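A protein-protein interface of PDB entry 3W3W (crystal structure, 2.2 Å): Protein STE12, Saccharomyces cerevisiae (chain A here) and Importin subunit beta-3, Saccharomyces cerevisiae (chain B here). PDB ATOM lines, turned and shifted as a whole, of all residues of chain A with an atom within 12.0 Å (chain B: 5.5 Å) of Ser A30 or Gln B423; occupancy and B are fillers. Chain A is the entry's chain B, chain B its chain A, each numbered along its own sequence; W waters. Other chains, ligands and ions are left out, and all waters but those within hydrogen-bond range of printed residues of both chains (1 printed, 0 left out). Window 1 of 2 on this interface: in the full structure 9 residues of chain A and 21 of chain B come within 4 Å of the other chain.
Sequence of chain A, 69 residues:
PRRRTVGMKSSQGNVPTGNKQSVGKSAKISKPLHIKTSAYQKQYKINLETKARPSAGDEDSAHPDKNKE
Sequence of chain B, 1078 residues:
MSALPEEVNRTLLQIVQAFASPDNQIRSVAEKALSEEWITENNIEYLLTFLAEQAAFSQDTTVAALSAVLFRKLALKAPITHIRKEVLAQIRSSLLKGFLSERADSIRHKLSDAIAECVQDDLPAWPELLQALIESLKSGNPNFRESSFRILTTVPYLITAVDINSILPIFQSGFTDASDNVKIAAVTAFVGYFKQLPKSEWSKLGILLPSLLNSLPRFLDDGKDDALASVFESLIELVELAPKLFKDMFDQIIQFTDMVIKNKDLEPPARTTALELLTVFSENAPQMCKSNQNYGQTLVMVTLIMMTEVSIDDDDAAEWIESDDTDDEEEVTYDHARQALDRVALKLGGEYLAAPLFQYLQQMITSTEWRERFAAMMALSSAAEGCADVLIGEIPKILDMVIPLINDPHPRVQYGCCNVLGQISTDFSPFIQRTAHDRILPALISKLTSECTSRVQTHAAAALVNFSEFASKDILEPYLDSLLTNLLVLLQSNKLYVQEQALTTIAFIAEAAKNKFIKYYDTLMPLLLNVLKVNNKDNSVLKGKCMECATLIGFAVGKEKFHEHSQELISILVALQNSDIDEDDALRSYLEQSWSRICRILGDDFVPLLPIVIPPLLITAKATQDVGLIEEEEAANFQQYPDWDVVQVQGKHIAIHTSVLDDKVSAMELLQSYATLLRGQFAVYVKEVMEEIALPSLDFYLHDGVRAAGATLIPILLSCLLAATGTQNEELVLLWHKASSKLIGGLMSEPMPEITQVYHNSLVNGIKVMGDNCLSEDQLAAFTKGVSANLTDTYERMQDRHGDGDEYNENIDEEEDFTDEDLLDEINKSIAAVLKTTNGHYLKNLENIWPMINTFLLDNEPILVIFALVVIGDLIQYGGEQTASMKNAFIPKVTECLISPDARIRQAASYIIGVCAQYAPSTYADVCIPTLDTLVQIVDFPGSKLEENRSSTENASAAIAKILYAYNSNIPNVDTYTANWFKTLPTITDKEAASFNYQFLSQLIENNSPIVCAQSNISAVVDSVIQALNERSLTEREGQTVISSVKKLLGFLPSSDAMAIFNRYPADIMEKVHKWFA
The backbone NH (N) of Ile A29 lies within hydrogen-bond range of the side-chain amide oxygen (OD1) of Asn B466, at 2.7 Å.
The backbone carbonyl oxygen (O) of Arg B338 is in hydrogen-bond range of the side-chain hydroxyl (OG) of Ser B382, 3.5 Å away. The side-chain amide nitrogen of Asn B419 lies within hydrogen-bond range of the side-chain hydroxyl of Ser B381 (3.0 Å). The side-chain amide nitrogen (ND2) of Asn B466 sits close to the backbone carbonyl oxygen (O) of Gly B422 (3.4 Å). The side-chain amide nitrogen (NE2) of Gln B423 lies within hydrogen-bond range of the side-chain carboxylate (OD2) of Asp B427 (2.7 Å). OG1 of Thr B426 sits at hydrogen-bond distance from ND2 of Asn B466 (2.7 Å).
Among the printed residues, pairs that only touch across the chains: Lys A28 with Asn B466 (3.4 Å), Pro A32 with Arg B338 (3.5 Å), Ile A29 with Asn B419 (3.5 Å), Lys A31 with Gln B423 (3.5 Å), Ser A30 with Gln B423 (3.7 Å), Ile A29 with Gln B423 (3.7 Å), Ile A29 with Gly B422 (3.8 Å) and Lys A31 with Ser B382 (3.99 Å).
Gln B423 touches just these residues of chain A: Ile A29 (3.7 Å), Ser A30 (3.7 Å) and Lys A31 (3.5 Å). No residue of chain A comes within 4 Å of Ala B384. Of chain A, only Ile A29 comes within 4 Å of Asn B419. No residue of chain A comes within 4 Å of Val B420. Gly B422 touches one residue of chain A. No residue of chain A comes within 4 Å of Ile B424. No residue of chain A comes within 4 Å of Ser B425. No residue of chain A comes within 4 Å of Thr B426. No residue of chain A comes within 4 Å of Asp B427. Asn B466 touches just these residues of chain A: Lys A28 and Ile A29. Of the printed residues of chain B, Lys A28 touches Asn B466. Of the printed residues of chain B, Pro A32 touches Arg B338. Of the printed residues of chain A, Ser B382 touches Lys A31 (3.99 Å). Printed residues of chain A within 4 Å of Arg B338: Pro A32 (3.5 Å). Of the printed residues of chain B, Ile A29 touches Asn B419 (3.5 Å), Gly B422 (3.8 Å), Gln B423 (3.7 Å) and Asn B466 (2.7 Å). The nearest residue of chain B that does not touch Ser A30 is Arg B338 (4.2 Å). The nearest residue of chain A that does not touch Gln B423 is Pro A32 (6.8 Å). The nearest printed residue of chain A that does not touch Arg B338 is Ser A30 (4.2 Å).
Of the 16 printed residues of chain B, 6 touch a printed residue of chain A. Printed residues of chain B that touch a printed residue of chain A: Arg B338, Ser B382, Asn B419, Gly B422, Gln B423 and Asn B466. Of the 9 printed residues of chain A, 5 touch a printed residue of chain B. Among the printed residues, 9 pairs touch across the chains.
Water W1 lies within hydrogen-bond range of OD2 of Asp B427 (2.8 Å), O of Ser B381 (2.8 Å), NZ of Lys A31 (3.3 Å) and N of Ala B384 (3.5 Å).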
ATOM      1  N   SER A  26      -9.807  17.675 -28.545  1.00  0.00           N
ATOM      2  CA  SER A  26      -8.353  17.275 -28.614  1.00  0.00           C
ATOM      3  C   SER A  26      -7.998  16.473 -29.854  1.00  0.00           C
ATOM      4  O   SER A  26      -8.529  15.382 -30.102  1.00  0.00           O
ATOM      5  CB  SER A  26      -7.881  16.456 -27.415  1.00  0.00           C
ATOM      6  OG  SER A  26      -6.480  16.623 -27.262  1.00  0.00           O
ATOM      7  N   ALA A  27      -7.065  17.009 -30.616  1.00  0.00           N
ATOM      8  CA  ALA A  27      -6.637  16.299 -31.790  1.00  0.00           C
ATOM      9  C   ALA A  27      -5.212  15.739 -31.559  1.00  0.00           C
ATOM     10  O   ALA A  27      -4.402  15.720 -32.453  1.00  0.00           O
ATOM     11  CB  ALA A  27      -6.721  17.199 -33.007  1.00  0.00           C
ATOM     12  N   LYS A  28      -4.928  15.338 -30.318  1.00  0.00           N
ATOM     13  CA  LYS A  28      -3.832  14.437 -30.031  1.00  0.00           C
ATOM     14  C   LYS A  28      -4.222  13.381 -28.947  1.00  0.00           C
ATOM     15  O   LYS A  28      -5.294  13.428 -28.405  1.00  0.00           O
ATOM     16  CB  LYS A  28      -2.610  15.255 -29.646  1.00  0.00           C
ATOM     17  CG  LYS A  28      -2.780  15.935 -28.311  1.00  0.00           C
ATOM     18  CD  LYS A  28      -1.443  16.532 -27.981  1.00  0.00           C
ATOM     19  CE  LYS A  28      -1.490  17.409 -26.762  1.00  0.00           C
ATOM     20  NZ  LYS A  28      -0.077  17.796 -26.492  1.00  0.00           N
ATOM     21  N   ILE A  29      -3.337  12.458 -28.599  1.00  0.00           N
ATOM     22  CA  ILE A  29      -3.640  11.569 -27.502  1.00  0.00           C
ATOM     23  C   ILE A  29      -3.460  12.332 -26.191  1.00  0.00           C
ATOM     24  O   ILE A  29      -2.470  13.054 -26.004  1.00  0.00           O
ATOM     25  CB  ILE A  29      -2.714  10.324 -27.502  1.00  0.00           C
ATOM     26  CG1 ILE A  29      -2.717   9.624 -28.893  1.00  0.00           C
ATOM     27  CG2 ILE A  29      -3.074   9.377 -26.387  1.00  0.00           C
ATOM     28  CD1 ILE A  29      -4.103   9.376 -29.433  1.00  0.00           C
ATOM     29  N   SER A  30      -4.404  12.145 -25.288  1.00  0.00           N
ATOM     30  CA  SER A  30      -4.301  12.677 -23.921  1.00  0.00           C
ATOM     31  C   SER A  30      -5.170  11.885 -22.975  1.00  0.00           C
ATOM     32  O   SER A  30      -6.039  11.139 -23.392  1.00  0.00           O
ATOM     33  CB  SER A  30      -4.756  14.147 -23.872  1.00  0.00           C
ATOM     34  OG  SER A  30      -6.102  14.278 -24.336  1.00  0.00           O
ATOM     35  N   LYS A  31      -4.946  12.044 -21.679  1.00  0.00           N
ATOM     36  CA  LYS A  31      -5.683  11.271 -20.708  1.00  0.00           C
ATOM     37  C   LYS A  31      -6.996  11.941 -20.284  1.00  0.00           C
ATOM     38  O   LYS A  31      -7.142  13.137 -20.371  1.00  0.00           O
ATOM     39  CB  LYS A  31      -4.834  11.059 -19.510  1.00  0.00           C
ATOM     40  CG  LYS A  31      -3.477  10.487 -19.827  1.00  0.00           C
ATOM     41  CD  LYS A  31      -2.844   9.959 -18.573  1.00  0.00           C
ATOM     42  CE  LYS A  31      -1.458  10.510 -18.600  1.00  0.00           C
ATOM     43  NZ  LYS A  31      -1.015  11.085 -17.352  1.00  0.00           N
ATOM     44  N   PRO A  32      -7.961  11.140 -19.825  1.00  0.00           N
ATOM     45  CA  PRO A  32      -9.239  11.683 -19.355  1.00  0.00           C
ATOM     46  C   PRO A  32      -9.009  12.548 -18.135  1.00  0.00           C
ATOM     47  O   PRO A  32      -8.030  12.327 -17.400  1.00  0.00           O
ATOM     48  CB  PRO A  32     -10.056  10.462 -18.947  1.00  0.00           C
ATOM     49  CG  PRO A  32      -9.306   9.275 -19.477  1.00  0.00           C
ATOM     50  CD  PRO A  32      -7.887   9.673 -19.741  1.00  0.00           C
ATOM     51  N   LEU A  33      -9.910  13.498 -17.940  1.00  0.00           N
ATOM     52  CA  LEU A  33      -9.838  14.466 -16.843  1.00  0.00           C
ATOM     53  C   LEU A  33     -10.028  13.806 -15.511  1.00  0.00           C
ATOM     54  O   LEU A  33     -10.789  12.871 -15.396  1.00  0.00           O
ATOM     55  CB  LEU A  33     -10.900  15.546 -17.051  1.00  0.00           C
ATOM     56  CG  LEU A  33     -10.197  16.914 -17.152  1.00  0.00           C
ATOM     57  CD1 LEU A  33      -9.312  17.102 -15.910  1.00  0.00           C
ATOM     58  CD2 LEU A  33      -9.374  17.092 -18.433  1.00  0.00           C
ATOM     59  N   HIS A  34      -9.347  14.279 -14.477  1.00  0.00           N
ATOM     60  CA  HIS A  34      -9.516  13.606 -13.171  1.00  0.00           C
ATOM     61  C   HIS A  34     -10.919  13.744 -12.593  1.00  0.00           C
ATOM     62  O   HIS A  34     -11.587  14.754 -12.831  1.00  0.00           O
ATOM     63  CB  HIS A  34      -8.454  13.990 -12.171  1.00  0.00           C
ATOM     64  CG  HIS A  34      -7.089  13.564 -12.601  1.00  0.00           C
ATOM     65  ND1 HIS A  34      -5.941  13.923 -11.927  1.00  0.00           N
ATOM     66  CD2 HIS A  34      -6.685  12.852 -13.686  1.00  0.00           C
ATOM     67  CE1 HIS A  34      -4.893  13.414 -12.554  1.00  0.00           C
ATOM     68  NE2 HIS A  34      -5.320  12.757 -13.624  1.00  0.00           N
ATOM     69  N   ARG B 338      -9.152   4.404 -15.877  1.00  0.00           N
ATOM     70  CA  ARG B 338      -8.013   5.090 -16.500  1.00  0.00           C
ATOM     71  C   ARG B 338      -7.544   6.288 -15.663  1.00  0.00           C
ATOM     72  O   ARG B 338      -6.374   6.447 -15.433  1.00  0.00           O
ATOM     73  CB  ARG B 338      -8.406   5.624 -17.888  1.00  0.00           C
ATOM     74  CG  ARG B 338      -8.752   4.542 -18.891  1.00  0.00           C
ATOM     75  CD  ARG B 338      -9.316   5.190 -20.144  1.00  0.00           C
ATOM     76  NE  ARG B 338      -8.258   5.892 -20.778  1.00  0.00           N
ATOM     77  CZ  ARG B 338      -8.410   6.772 -21.777  1.00  0.00           C
ATOM     78  NH1 ARG B 338      -9.583   7.059 -22.289  1.00  0.00           N
ATOM     79  NH2 ARG B 338      -7.339   7.337 -22.268  1.00  0.00           N
ATOM     80  N   SER B 381      -0.799   3.509 -20.999  1.00  0.00           N
ATOM     81  CA  SER B 381      -1.091   4.824 -21.390  1.00  0.00           C
ATOM     82  C   SER B 381      -1.386   5.631 -20.137  1.00  0.00           C
ATOM     83  O   SER B 381      -0.871   6.741 -20.010  1.00  0.00           O
ATOM     84  CB  SER B 381      -2.300   4.835 -22.301  1.00  0.00           C
ATOM     85  OG  SER B 381      -1.960   4.399 -23.595  1.00  0.00           O
ATOM     86  N   SER B 382      -2.188   5.074 -19.206  1.00  0.00           N
ATOM     87  CA  SER B 382      -2.524   5.805 -17.970  1.00  0.00           C
ATOM     88  C   SER B 382      -1.356   5.999 -17.007  1.00  0.00           C
ATOM     89  O   SER B 382      -1.221   7.077 -16.344  1.00  0.00           O
ATOM     90  CB  SER B 382      -3.690   5.169 -17.240  1.00  0.00           C
ATOM     91  OG  SER B 382      -4.795   4.939 -18.133  1.00  0.00           O
ATOM     92  N   ALA B 384       2.023   5.721 -17.726  1.00  0.00           N
ATOM     93  CA  ALA B 384       3.366   6.069 -18.222  1.00  0.00           C
ATOM     94  C   ALA B 384       3.894   7.343 -17.638  1.00  0.00           C
ATOM     95  O   ALA B 384       5.063   7.417 -17.357  1.00  0.00           O
ATOM     96  CB  ALA B 384       3.358   6.196 -19.713  1.00  0.00           C
ATOM     97  N   CYS B 418      -1.985   2.633 -30.871  1.00  0.00           N
ATOM     98  CA  CYS B 418      -1.802   3.982 -31.365  1.00  0.00           C
ATOM     99  C   CYS B 418      -1.811   4.901 -30.159  1.00  0.00           C
ATOM    100  O   CYS B 418      -0.930   5.714 -29.975  1.00  0.00           O
ATOM    101  CB  CYS B 418      -2.938   4.311 -32.331  1.00  0.00           C
ATOM    102  SG  CYS B 418      -2.783   3.508 -33.959  1.00  0.00           S
ATOM    103  N   ASN B 419      -2.736   4.632 -29.250  1.00  0.00           N
ATOM    104  CA  ASN B 419      -2.903   5.428 -28.040  1.00  0.00           C
ATOM    105  C   ASN B 419      -1.659   5.431 -27.224  1.00  0.00           C
ATOM    106  O   ASN B 419      -1.161   6.500 -26.862  1.00  0.00           O
ATOM    107  CB  ASN B 419      -4.126   4.962 -27.242  1.00  0.00           C
ATOM    108  CG  ASN B 419      -4.567   6.005 -26.231  1.00  0.00           C
ATOM    109  OD1 ASN B 419      -5.420   6.799 -26.545  1.00  0.00           O
ATOM    110  ND2 ASN B 419      -3.961   6.027 -25.061  1.00  0.00           N
ATOM    111  N   VAL B 420      -1.068   4.262 -27.005  1.00  0.00           N
ATOM    112  CA  VAL B 420       0.133   4.267 -26.207  1.00  0.00           C
ATOM    113  C   VAL B 420       1.297   4.905 -26.874  1.00  0.00           C
ATOM    114  O   VAL B 420       2.105   5.568 -26.194  1.00  0.00           O
ATOM    115  CB  VAL B 420       0.675   2.883 -25.902  1.00  0.00           C
ATOM    116  CG1 VAL B 420       1.352   2.923 -24.527  1.00  0.00           C
ATOM    117  CG2 VAL B 420      -0.422   1.884 -25.948  1.00  0.00           C
ATOM    118  N   LEU B 421       1.464   4.664 -28.189  1.00  0.00           N
ATOM    119  CA  LEU B 421       2.633   5.286 -28.848  1.00  0.00           C
ATOM    120  C   LEU B 421       2.511   6.807 -28.768  1.00  0.00           C
ATOM    121  O   LEU B 421       3.499   7.508 -28.532  1.00  0.00           O
ATOM    122  CB  LEU B 421       2.762   4.787 -30.297  1.00  0.00           C
ATOM    123  CG  LEU B 421       3.037   3.255 -30.381  1.00  0.00           C
ATOM    124  CD1 LEU B 421       2.940   2.695 -31.800  1.00  0.00           C
ATOM    125  CD2 LEU B 421       4.367   2.831 -29.770  1.00  0.00           C
ATOM    126  N   GLY B 422       1.273   7.290 -28.946  1.00  0.00           N
ATOM    127  CA  GLY B 422       1.004   8.693 -28.708  1.00  0.00           C
ATOM    128  C   GLY B 422       1.269   9.136 -27.257  1.00  0.00           C
ATOM    129  O   GLY B 422       1.977  10.109 -27.032  1.00  0.00           O
ATOM    130  N   GLN B 423       0.771   8.394 -26.265  1.00  0.00           N
ATOM    131  CA  GLN B 423       0.929   8.879 -24.866  1.00  0.00           C
ATOM    132  C   GLN B 423       2.377   8.941 -24.447  1.00  0.00           C
ATOM    133  O   GLN B 423       2.837   9.912 -23.797  1.00  0.00           O
ATOM    134  CB  GLN B 423       0.094   8.015 -23.897  1.00  0.00           C
ATOM    135  CG  GLN B 423      -0.023   8.614 -22.499  1.00  0.00           C
ATOM    136  CD  GLN B 423      -0.733   9.956 -22.498  1.00  0.00           C
ATOM    137  OE1 GLN B 423      -1.885  10.080 -22.957  1.00  0.00           O
ATOM    138  NE2 GLN B 423      -0.020  10.990 -22.037  1.00  0.00           N
ATOM    139  N   ILE B 424       3.141   7.938 -24.876  1.00  0.00           N
ATOM    140  CA  ILE B 424       4.525   7.937 -24.469  1.00  0.00           C
ATOM    141  C   ILE B 424       5.347   8.869 -25.292  1.00  0.00           C
ATOM    142  O   ILE B 424       6.349   9.342 -24.814  1.00  0.00           O
ATOM    143  CB  ILE B 424       5.171   6.567 -24.408  1.00  0.00           C
ATOM    144  CG1 ILE B 424       5.357   5.995 -25.815  1.00  0.00           C
ATOM    145  CG2 ILE B 424       4.321   5.642 -23.543  1.00  0.00           C
ATOM    146  CD1 ILE B 424       5.856   4.567 -25.803  1.00  0.00           C
ATOM    147  N   SER B 425       4.945   9.186 -26.519  1.00  0.00           N
ATOM    148  CA  SER B 425       5.714  10.253 -27.215  1.00  0.00           C
ATOM    149  C   SER B 425       5.631  11.568 -26.429  1.00  0.00           C
ATOM    150  O   SER B 425       6.536  12.393 -26.496  1.00  0.00           O
ATOM    151  CB  SER B 425       5.230  10.446 -28.655  1.00  0.00           C
ATOM    152  OG  SER B 425       5.353   9.223 -29.379  1.00  0.00           O
ATOM    153  N   THR B 426       4.553  11.753 -25.661  1.00  0.00           N
ATOM    154  CA  THR B 426       4.499  12.904 -24.839  1.00  0.00           C
ATOM    155  C   THR B 426       5.263  12.700 -23.554  1.00  0.00           C
ATOM    156  O   THR B 426       6.072  13.526 -23.161  1.00  0.00           O
ATOM    157  CB  THR B 426       3.055  13.224 -24.448  1.00  0.00           C
ATOM    158  OG1 THR B 426       2.322  13.482 -25.651  1.00  0.00           O
ATOM    159  CG2 THR B 426       3.008  14.478 -23.512  1.00  0.00           C
ATOM    160  N   ASP B 427       4.966  11.606 -22.878  1.00  0.00           N
ATOM    161  CA  ASP B 427       5.451  11.426 -21.526  1.00  0.00           C
ATOM    162  C   ASP B 427       6.916  11.128 -21.435  1.00  0.00           C
ATOM    163  O   ASP B 427       7.478  11.395 -20.425  1.00  0.00           O
ATOM    164  CB  ASP B 427       4.592  10.375 -20.796  1.00  0.00           C
ATOM    165  CG  ASP B 427       3.139  10.861 -20.636  1.00  0.00           C
ATOM    166  OD1 ASP B 427       2.907  12.064 -20.357  1.00  0.00           O
ATOM    167  OD2 ASP B 427       2.214  10.061 -20.771  1.00  0.00           O
ATOM    168  N   PHE B 428       7.529  10.517 -22.463  1.00  0.00           N
ATOM    169  CA  PHE B 428       8.982  10.242 -22.438  1.00  0.00           C
ATOM    170  C   PHE B 428       9.775  11.190 -23.352  1.00  0.00           C
ATOM    171  O   PHE B 428      10.920  10.909 -23.690  1.00  0.00           O
ATOM    172  CB  PHE B 428       9.263   8.793 -22.823  1.00  0.00           C
ATOM    173  CG  PHE B 428       8.499   7.748 -22.012  1.00  0.00           C
ATOM    174  CD1 PHE B 428       8.023   8.011 -20.740  1.00  0.00           C
ATOM    175  CD2 PHE B 428       8.363   6.469 -22.494  1.00  0.00           C
ATOM    176  CE1 PHE B 428       7.353   7.017 -20.014  1.00  0.00           C
ATOM    177  CE2 PHE B 428       7.687   5.457 -21.784  1.00  0.00           C
ATOM    178  CZ  PHE B 428       7.171   5.729 -20.537  1.00  0.00           C
ATOM    179  N   ASN B 466       1.308  13.939 -30.987  1.00  0.00           N
ATOM    180  CA  ASN B 466       2.114  13.814 -29.801  1.00  0.00           C
ATOM    181  C   ASN B 466       3.557  13.651 -30.177  1.00  0.00           C
ATOM    182  O   ASN B 466       4.445  14.322 -29.588  1.00  0.00           O
ATOM    183  CB  ASN B 466       1.711  12.640 -28.937  1.00  0.00           C
ATOM    184  CG  ASN B 466       0.286  12.707 -28.441  1.00  0.00           C
ATOM    185  OD1 ASN B 466      -0.662  12.449 -29.197  1.00  0.00           O
ATOM    186  ND2 ASN B 466       0.116  12.984 -27.144  1.00  0.00           N
HETATM  187  O   HOH W   1       0.717   8.767 -18.838  1.00  0.00           O
